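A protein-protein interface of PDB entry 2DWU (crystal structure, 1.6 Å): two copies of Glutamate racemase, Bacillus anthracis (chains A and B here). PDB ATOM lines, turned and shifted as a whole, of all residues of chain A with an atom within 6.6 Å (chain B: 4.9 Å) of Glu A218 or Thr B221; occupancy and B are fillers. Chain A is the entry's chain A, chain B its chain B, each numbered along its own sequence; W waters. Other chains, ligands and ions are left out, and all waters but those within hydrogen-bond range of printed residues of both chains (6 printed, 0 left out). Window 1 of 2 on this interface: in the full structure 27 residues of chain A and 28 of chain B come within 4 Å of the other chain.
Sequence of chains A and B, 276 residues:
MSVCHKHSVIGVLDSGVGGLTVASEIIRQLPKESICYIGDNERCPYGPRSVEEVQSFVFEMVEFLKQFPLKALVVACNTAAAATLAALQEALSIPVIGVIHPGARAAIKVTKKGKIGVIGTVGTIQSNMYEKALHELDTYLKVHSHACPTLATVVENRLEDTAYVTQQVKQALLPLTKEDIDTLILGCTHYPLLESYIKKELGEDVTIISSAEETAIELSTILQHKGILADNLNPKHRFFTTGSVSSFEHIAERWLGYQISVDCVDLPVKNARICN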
ATOM      1  N   GLN A  29      11.536  19.596  10.182  1.00  0.00           N
ATOM      2  CA  GLN A  29      11.209  18.179  10.348  1.00  0.00           C
ATOM      3  C   GLN A  29      11.571  17.294   9.153  1.00  0.00           C
ATOM      4  O   GLN A  29      11.677  16.074   9.283  1.00  0.00           O
ATOM      5  CB  GLN A  29       9.711  18.044  10.652  1.00  0.00           C
ATOM      6  CG  GLN A  29       9.290  18.740  11.925  1.00  0.00           C
ATOM      7  CD  GLN A  29       7.832  18.457  12.239  1.00  0.00           C
ATOM      8  OE1 GLN A  29       7.428  17.303  12.239  1.00  0.00           O
ATOM      9  NE2 GLN A  29       7.037  19.504  12.474  1.00  0.00           N
ATOM     10  N   ILE A  97      -1.152  17.951   0.206  1.00  0.00           N
ATOM     11  CA  ILE A  97      -1.353  18.019   1.649  1.00  0.00           C
ATOM     12  C   ILE A  97      -1.793  19.429   2.019  1.00  0.00           C
ATOM     13  O   ILE A  97      -1.086  20.398   1.721  1.00  0.00           O
ATOM     14  CB  ILE A  97      -0.024  17.712   2.435  1.00  0.00           C
ATOM     15  CG1 ILE A  97       0.343  16.221   2.354  1.00  0.00           C
ATOM     16  CG2 ILE A  97      -0.187  18.054   3.903  1.00  0.00           C
ATOM     17  CD1 ILE A  97       0.875  15.778   1.008  1.00  0.00           C
ATOM     18  N   GLY A  98      -2.967  19.545   2.635  1.00  0.00           N
ATOM     19  CA  GLY A  98      -3.461  20.849   3.075  1.00  0.00           C
ATOM     20  C   GLY A  98      -3.174  20.992   4.561  1.00  0.00           C
ATOM     21  O   GLY A  98      -2.822  20.009   5.229  1.00  0.00           O
ATOM     22  N   HIS A 101      -6.587  19.337   7.599  1.00  0.00           N
ATOM     23  CA  HIS A 101      -6.708  17.981   8.125  1.00  0.00           C
ATOM     24  C   HIS A 101      -5.635  17.587   9.126  1.00  0.00           C
ATOM     25  O   HIS A 101      -5.933  16.914  10.112  1.00  0.00           O
ATOM     26  CB  HIS A 101      -6.802  16.958   6.983  1.00  0.00           C
ATOM     27  CG  HIS A 101      -8.076  17.070   6.201  1.00  0.00           C
ATOM     28  ND1 HIS A 101      -8.301  18.068   5.279  1.00  0.00           N
ATOM     29  CD2 HIS A 101      -9.231  16.366   6.281  1.00  0.00           C
ATOM     30  CE1 HIS A 101      -9.541  17.977   4.822  1.00  0.00           C
ATOM     31  NE2 HIS A 101     -10.129  16.950   5.413  1.00  0.00           N
ATOM     32  N   PRO A 102      -4.376  18.010   8.914  1.00  0.00           N
ATOM     33  CA  PRO A 102      -3.349  17.634   9.894  1.00  0.00           C
ATOM     34  C   PRO A 102      -3.653  18.240  11.269  1.00  0.00           C
ATOM     35  O   PRO A 102      -3.409  17.601  12.316  1.00  0.00           O
ATOM     36  CB  PRO A 102      -2.061  18.215   9.281  1.00  0.00           C
ATOM     37  CG  PRO A 102      -2.310  18.041   7.824  1.00  0.00           C
ATOM     38  CD  PRO A 102      -3.760  18.570   7.696  1.00  0.00           C
ATOM     39  N   GLY A 103      -4.168  19.472  11.262  1.00  0.00           N
ATOM     40  CA  GLY A 103      -4.524  20.149  12.506  1.00  0.00           C
ATOM     41  C   GLY A 103      -5.686  19.426  13.199  1.00  0.00           C
ATOM     42  O   GLY A 103      -5.661  19.219  14.405  1.00  0.00           O
ATOM     43  N   ARG A 105      -6.525  16.291  12.902  1.00  0.00           N
ATOM     44  CA  ARG A 105      -6.032  15.002  13.374  1.00  0.00           C
ATOM     45  C   ARG A 105      -5.260  15.138  14.685  1.00  0.00           C
ATOM     46  O   ARG A 105      -5.395  14.319  15.604  1.00  0.00           O
ATOM     47  CB  ARG A 105      -5.123  14.384  12.292  1.00  0.00           C
ATOM     48  CG  ARG A 105      -5.091  12.864  12.358  1.00  0.00           C
ATOM     49  CD  ARG A 105      -4.108  12.305  11.282  1.00  0.00           C
ATOM     50  NE  ARG A 105      -4.306  12.910   9.960  1.00  0.00           N
ATOM     51  CZ  ARG A 105      -5.359  12.704   9.165  1.00  0.00           C
ATOM     52  NH1 ARG A 105      -6.354  11.886   9.525  1.00  0.00           N
ATOM     53  NH2 ARG A 105      -5.449  13.366   8.015  1.00  0.00           N
ATOM     54  N   ALA A 106      -4.413  16.163  14.774  1.00  0.00           N
ATOM     55  CA  ALA A 106      -3.635  16.387  15.981  1.00  0.00           C
ATOM     56  C   ALA A 106      -4.564  16.776  17.134  1.00  0.00           C
ATOM     57  O   ALA A 106      -4.300  16.451  18.275  1.00  0.00           O
ATOM     58  CB  ALA A 106      -2.609  17.507  15.739  1.00  0.00           C
ATOM     59  N   GLU A 213       3.265  22.900  12.434  1.00  0.00           N
ATOM     60  CA  GLU A 213       3.916  21.738  13.037  1.00  0.00           C
ATOM     61  C   GLU A 213       3.241  20.448  12.632  1.00  0.00           C
ATOM     62  O   GLU A 213       3.903  19.472  12.328  1.00  0.00           O
ATOM     63  CB  GLU A 213       3.866  21.807  14.569  1.00  0.00           C
ATOM     64  CG  GLU A 213       4.459  23.034  15.165  1.00  0.00           C
ATOM     65  CD  GLU A 213       4.650  22.879  16.662  1.00  0.00           C
ATOM     66  OE1 GLU A 213       3.836  22.158  17.295  1.00  0.00           O
ATOM     67  OE2 GLU A 213       5.609  23.478  17.200  1.00  0.00           O
ATOM     68  N   GLU A 214       1.910  20.444  12.617  1.00  0.00           N
ATOM     69  CA  GLU A 214       1.227  19.202  12.277  1.00  0.00           C
ATOM     70  C   GLU A 214       1.239  18.881  10.794  1.00  0.00           C
ATOM     71  O   GLU A 214       1.215  17.715  10.405  1.00  0.00           O
ATOM     72  CB  GLU A 214      -0.205  19.281  12.792  1.00  0.00           C
ATOM     73  CG  GLU A 214      -0.256  19.726  14.254  1.00  0.00           C
ATOM     74  CD  GLU A 214       0.516  18.827  15.211  1.00  0.00           C
ATOM     75  OE1 GLU A 214       0.822  17.676  14.852  1.00  0.00           O
ATOM     76  OE2 GLU A 214       0.784  19.274  16.347  1.00  0.00           O
ATOM     77  N   THR A 215       1.303  19.907   9.948  1.00  0.00           N
ATOM     78  CA  THR A 215       1.293  19.645   8.511  1.00  0.00           C
ATOM     79  C   THR A 215       2.626  19.045   8.094  1.00  0.00           C
ATOM     80  O   THR A 215       2.677  18.178   7.218  1.00  0.00           O
ATOM     81  CB  THR A 215       0.993  20.939   7.732  1.00  0.00           C
ATOM     82  OG1 THR A 215      -0.350  21.327   8.028  1.00  0.00           O
ATOM     83  CG2 THR A 215       1.062  20.726   6.221  1.00  0.00           C
ATOM     84  N   ALA A 216       3.695  19.471   8.745  1.00  0.00           N
ATOM     85  CA  ALA A 216       4.999  18.931   8.384  1.00  0.00           C
ATOM     86  C   ALA A 216       5.089  17.448   8.735  1.00  0.00           C
ATOM     87  O   ALA A 216       5.604  16.643   7.941  1.00  0.00           O
ATOM     88  CB  ALA A 216       6.126  19.727   9.085  1.00  0.00           C
ATOM     89  N   ILE A 217       4.555  17.056   9.896  1.00  0.00           N
ATOM     90  CA  ILE A 217       4.639  15.652  10.240  1.00  0.00           C
ATOM     91  C   ILE A 217       3.686  14.857   9.354  1.00  0.00           C
ATOM     92  O   ILE A 217       3.976  13.732   9.000  1.00  0.00           O
ATOM     93  CB  ILE A 217       4.432  15.396  11.768  1.00  0.00           C
ATOM     94  CG1 ILE A 217       4.738  13.922  12.087  1.00  0.00           C
ATOM     95  CG2 ILE A 217       3.039  15.828  12.221  1.00  0.00           C
ATOM     96  CD1 ILE A 217       5.031  13.711  13.573  1.00  0.00           C
ATOM     97  N   GLU A 218       2.565  15.452   8.937  1.00  0.00           N
ATOM     98  CA  GLU A 218       1.657  14.739   8.043  1.00  0.00           C
ATOM     99  C   GLU A 218       2.350  14.495   6.701  1.00  0.00           C
ATOM    100  O   GLU A 218       2.280  13.408   6.133  1.00  0.00           O
ATOM    101  CB  GLU A 218       0.372  15.543   7.813  1.00  0.00           C
ATOM    102  CG  GLU A 218      -0.634  14.820   6.937  1.00  0.00           C
ATOM    103  CD  GLU A 218      -2.006  14.514   7.594  1.00  0.00           C
ATOM    104  OE1 GLU A 218      -2.157  14.470   8.836  1.00  0.00           O
ATOM    105  OE2 GLU A 218      -2.951  14.292   6.799  1.00  0.00           O
ATOM    106  N   LEU A 219       3.027  15.524   6.201  1.00  0.00           N
ATOM    107  CA  LEU A 219       3.770  15.390   4.944  1.00  0.00           C
ATOM    108  C   LEU A 219       4.850  14.294   5.091  1.00  0.00           C
ATOM    109  O   LEU A 219       5.020  13.426   4.206  1.00  0.00           O
ATOM    110  CB  LEU A 219       4.436  16.736   4.586  1.00  0.00           C
ATOM    111  CG  LEU A 219       5.339  16.689   3.344  1.00  0.00           C
ATOM    112  CD1 LEU A 219       4.528  16.337   2.092  1.00  0.00           C
ATOM    113  CD2 LEU A 219       6.011  18.050   3.185  1.00  0.00           C
ATOM    114  N   SER A 220       5.592  14.339   6.189  1.00  0.00           N
ATOM    115  CA  SER A 220       6.610  13.333   6.449  1.00  0.00           C
ATOM    116  C   SER A 220       6.013  11.916   6.387  1.00  0.00           C
ATOM    117  O   SER A 220       6.546  11.040   5.748  1.00  0.00           O
ATOM    118  CB  SER A 220       7.260  13.618   7.818  1.00  0.00           C
ATOM    119  OG  SER A 220       8.234  12.626   8.141  1.00  0.00           O
ATOM    120  N   THR A 221       4.883  11.725   7.057  1.00  0.00           N
ATOM    121  CA  THR A 221       4.228  10.433   7.087  1.00  0.00           C
ATOM    122  C   THR A 221       3.881   9.942   5.688  1.00  0.00           C
ATOM    123  O   THR A 221       4.104   8.762   5.345  1.00  0.00           O
ATOM    124  CB  THR A 221       2.926  10.528   7.897  1.00  0.00           C
ATOM    125  OG1 THR A 221       3.221  10.944   9.230  1.00  0.00           O
ATOM    126  CG2 THR A 221       2.223   9.151   7.946  1.00  0.00           C
ATOM    127  N   ILE A 222       3.320  10.838   4.877  1.00  0.00           N
ATOM    128  CA  ILE A 222       2.902  10.457   3.533  1.00  0.00           C
ATOM    129  C   ILE A 222       4.072  10.224   2.611  1.00  0.00           C
ATOM    130  O   ILE A 222       4.047   9.276   1.824  1.00  0.00           O
ATOM    131  CB  ILE A 222       1.936  11.520   2.958  1.00  0.00           C
ATOM    132  CG1 ILE A 222       0.607  11.468   3.733  1.00  0.00           C
ATOM    133  CG2 ILE A 222       1.606  11.221   1.492  1.00  0.00           C
ATOM    134  CD1 ILE A 222      -0.254  12.721   3.526  1.00  0.00           C
ATOM    135  N   LEU A 223       5.103  11.057   2.687  1.00  0.00           N
ATOM    136  CA  LEU A 223       6.249  10.831   1.802  1.00  0.00           C
ATOM    137  C   LEU A 223       6.891   9.486   2.133  1.00  0.00           C
ATOM    138  O   LEU A 223       7.298   8.756   1.237  1.00  0.00           O
ATOM    139  CB  LEU A 223       7.298  11.933   1.946  1.00  0.00           C
ATOM    140  CG  LEU A 223       6.839  13.333   1.530  1.00  0.00           C
ATOM    141  CD1 LEU A 223       7.966  14.327   1.851  1.00  0.00           C
ATOM    142  CD2 LEU A 223       6.439  13.342   0.047  1.00  0.00           C
ATOM    143  N   ILE B 217      -2.081   8.036  15.305  1.00  0.00           N
ATOM    144  CA  ILE B 217      -2.236   9.168  14.416  1.00  0.00           C
ATOM    145  C   ILE B 217      -1.583   8.855  13.058  1.00  0.00           C
ATOM    146  O   ILE B 217      -2.070   9.291  12.028  1.00  0.00           O
ATOM    147  CB  ILE B 217      -1.730  10.491  15.062  1.00  0.00           C
ATOM    148  CG1 ILE B 217      -2.141  11.664  14.174  1.00  0.00           C
ATOM    149  CG2 ILE B 217      -0.226  10.442  15.341  1.00  0.00           C
ATOM    150  CD1 ILE B 217      -2.058  13.002  14.886  1.00  0.00           C
ATOM    151  N   GLU B 218      -0.513   8.052  13.043  1.00  0.00           N
ATOM    152  CA  GLU B 218       0.109   7.672  11.780  1.00  0.00           C
ATOM    153  C   GLU B 218      -0.877   6.832  10.958  1.00  0.00           C
ATOM    154  O   GLU B 218      -1.048   7.036   9.761  1.00  0.00           O
ATOM    155  CB  GLU B 218       1.397   6.871  12.030  1.00  0.00           C
ATOM    156  CG  GLU B 218       2.126   6.503  10.739  1.00  0.00           C
ATOM    157  CD  GLU B 218       3.548   7.077  10.606  1.00  0.00           C
ATOM    158  OE1 GLU B 218       3.928   8.078  11.264  1.00  0.00           O
ATOM    159  OE2 GLU B 218       4.291   6.500   9.785  1.00  0.00           O
ATOM    160  N   LEU B 219      -1.533   5.878  11.612  1.00  0.00           N
ATOM    161  CA  LEU B 219      -2.542   5.059  10.932  1.00  0.00           C
ATOM    162  C   LEU B 219      -3.670   5.963  10.392  1.00  0.00           C
ATOM    163  O   LEU B 219      -4.101   5.814   9.237  1.00  0.00           O
ATOM    164  CB  LEU B 219      -3.131   4.036  11.922  1.00  0.00           C
ATOM    165  CG  LEU B 219      -4.282   3.179  11.386  1.00  0.00           C
ATOM    166  CD1 LEU B 219      -3.803   2.312  10.215  1.00  0.00           C
ATOM    167  CD2 LEU B 219      -4.829   2.326  12.515  1.00  0.00           C
ATOM    168  N   SER B 220      -4.143   6.894  11.225  1.00  0.00           N
ATOM    169  CA  SER B 220      -5.202   7.816  10.808  1.00  0.00           C
ATOM    170  C   SER B 220      -4.797   8.570   9.515  1.00  0.00           C
ATOM    171  O   SER B 220      -5.566   8.658   8.548  1.00  0.00           O
ATOM    172  CB  SER B 220      -5.521   8.797  11.968  1.00  0.00           C
ATOM    173  OG  SER B 220      -6.518   9.741  11.572  1.00  0.00           O
ATOM    174  N   THR B 221      -3.570   9.078   9.498  1.00  0.00           N
ATOM    175  CA  THR B 221      -3.053   9.820   8.377  1.00  0.00           C
ATOM    176  C   THR B 221      -3.067   8.974   7.100  1.00  0.00           C
ATOM    177  O   THR B 221      -3.510   9.425   6.037  1.00  0.00           O
ATOM    178  CB  THR B 221      -1.590  10.260   8.668  1.00  0.00           C
ATOM    179  OG1 THR B 221      -1.548  11.075   9.845  1.00  0.00           O
ATOM    180  CG2 THR B 221      -1.032  11.034   7.471  1.00  0.00           C
ATOM    181  N   ILE B 222      -2.598   7.736   7.215  1.00  0.00           N
ATOM    182  CA  ILE B 222      -2.518   6.861   6.068  1.00  0.00           C
ATOM    183  C   ILE B 222      -3.888   6.401   5.595  1.00  0.00           C
ATOM    184  O   ILE B 222      -4.153   6.374   4.394  1.00  0.00           O
ATOM    185  CB  ILE B 222      -1.600   5.658   6.371  1.00  0.00           C
ATOM    186  CG1 ILE B 222      -0.150   6.148   6.486  1.00  0.00           C
ATOM    187  CG2 ILE B 222      -1.633   4.642   5.207  1.00  0.00           C
ATOM    188  CD1 ILE B 222       0.773   5.105   7.144  1.00  0.00           C
ATOM    189  N   LEU B 223      -4.776   6.043   6.515  1.00  0.00           N
ATOM    190  CA  LEU B 223      -6.106   5.609   6.074  1.00  0.00           C
ATOM    191  C   LEU B 223      -6.802   6.759   5.347  1.00  0.00           C
ATOM    192  O   LEU B 223      -7.450   6.537   4.330  1.00  0.00           O
ATOM    193  CB  LEU B 223      -6.975   5.180   7.260  1.00  0.00           C
ATOM    194  CG  LEU B 223      -6.527   3.950   8.067  1.00  0.00           C
ATOM    195  CD1 LEU B 223      -7.479   3.756   9.283  1.00  0.00           C
ATOM    196  CD2 LEU B 223      -6.501   2.723   7.158  1.00  0.00           C
ATOM    197  N   GLN B 224      -6.671   7.985   5.848  1.00  0.00           N
ATOM    198  CA  GLN B 224      -7.353   9.077   5.164  1.00  0.00           C
ATOM    199  C   GLN B 224      -6.697   9.401   3.823  1.00  0.00           C
ATOM    200  O   GLN B 224      -7.394   9.679   2.839  1.00  0.00           O
ATOM    201  CB  GLN B 224      -7.430  10.307   6.061  1.00  0.00           C
ATOM    202  CG  GLN B 224      -8.285  11.434   5.451  1.00  0.00           C
ATOM    203  CD  GLN B 224      -8.862  12.326   6.518  1.00  0.00           C
ATOM    204  OE1 GLN B 224      -8.236  12.560   7.547  1.00  0.00           O
ATOM    205  NE2 GLN B 224     -10.063  12.852   6.271  1.00  0.00           N
ATOM    206  N   HIS B 225      -5.369   9.340   3.772  1.00  0.00           N
ATOM    207  CA  HIS B 225      -4.654   9.590   2.520  1.00  0.00           C
ATOM    208  C   HIS B 225      -5.132   8.620   1.448  1.00  0.00           C
ATOM    209  O   HIS B 225      -5.321   8.999   0.275  1.00  0.00           O
ATOM    210  CB  HIS B 225      -3.151   9.393   2.745  1.00  0.00           C
ATOM    211  CG  HIS B 225      -2.366   9.286   1.477  1.00  0.00           C
ATOM    212  ND1 HIS B 225      -2.235  10.331   0.593  1.00  0.00           N
ATOM    213  CD2 HIS B 225      -1.700   8.240   0.926  1.00  0.00           C
ATOM    214  CE1 HIS B 225      -1.524   9.941  -0.446  1.00  0.00           C
ATOM    215  NE2 HIS B 225      -1.187   8.675  -0.270  1.00  0.00           N
HETATM  216  O   HOH W   1       2.795  10.126  12.359  1.00  0.00           O
HETATM  217  O   HOH W   2      -3.788  12.177   5.289  1.00  0.00           O
HETATM  218  O   HOH W   3       1.014  11.534  10.819  1.00  0.00           O
HETATM  219  O   HOH W   4       4.510   6.474   6.988  1.00  0.00           O
HETATM  220  O   HOH W   5      -8.014  14.879   9.331  1.00  0.00           O
HETATM  221  O   HOH W   6      -0.533  14.080  10.770  1.00  0.00           O
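NE of Arg A105 is in salt-bridge range of OE1 of Glu A218 (2.9 Å). The backbone carbonyl oxygen (O) of Ile A217 is in hydrogen-bond range of the side-chain hydroxyl (OG1) of Thr A221. O of Ile B217 sits at hydrogen-bond distance from OG1 of Thr B221 (2.9 Å).
Among the printed residues, pairs that only touch across the chains: His A101 with Gln B224, Arg A105 with Ile B217, Ala A106 with Ile B217, Glu A218 with Thr B221, Thr A221 with Glu B218, Thr A221 with Thr B221 and Ile A222 with His B225.
Glu A218 touches Thr B221, and with the chains exchanged Thr A221 touches Glu B218. Thr A221 touches its own counterpart, Thr B221. Positions printed for both chains: 217, 218, 219, 220, 221, 222 and 223. Of the 10 pairs that touch across the chains among the printed residues, 3 have their exchanged pair printed and touching as well.
The guanidinium group (NH1) of Arg A105 sits at hydrogen-bond distance from the side-chain hydroxyl (OG) of Ser B220, 3.0 Å away. The guanidinium group of Arg A105 sits close to the side-chain hydroxyl of Thr B221, 3.3 Å away. NH1 of Arg A105 lies within hydrogen-bond range of OE1 of Gln B224 (2.8 Å).
Water W6 bridges the side-chain carboxylate (OE1) of Glu A218 and the side-chain hydroxyl (OG1) of Thr B221. Water W1 lies within hydrogen-bond range of OE1 of Glu B218 (2.6 Å) and OG1 of Thr A221 (3.3 Å). Water W2 lies within hydrogen-bond range of the side-chain carboxylate (OE2) of Glu A218 (2.7 Å), the backbone carbonyl oxygen (O) of Thr B221 (2.9 Å) and the guanidinium group (NH2) of Arg A105 (3.4 Å). Water W3 bridges OG1 of Thr B221 (2.8 Å) and OG1 of Thr A221 (2.8 Å). Water W4 lies within hydrogen-bond range of OE2 of Glu B218 and O of Thr A221. Water W5 lies within hydrogen-bond range of the side-chain amide oxygen of Gln B224 (2.9 Å), the backbone carbonyl oxygen of His A101 (3.0 Å) and the guanidinium group of Arg A105 (3.3 Å).
Of the 9 printed residues of chain B, 6 touch a printed residue of chain A. Hydrophobic or aromatic side chains of chain A that line the printed part of chain B: His A101 and Ile A222. Along chain A the printed residues that touch a printed residue of chain B span positions 101 to 222. Among the printed residues, no Asp or Glu carboxylate lies within 4 Å of a Lys or Arg side-chain nitrogen of the other chain.
Of the printed residues of chain A, Glu B218 touches Thr A221. Of the printed residues of chain B, Ile A222 touches His B225 (3.9 Å). Glu A214 touches none of the printed residues of chain B. Ile B222 touches none of the printed residues of chain A.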
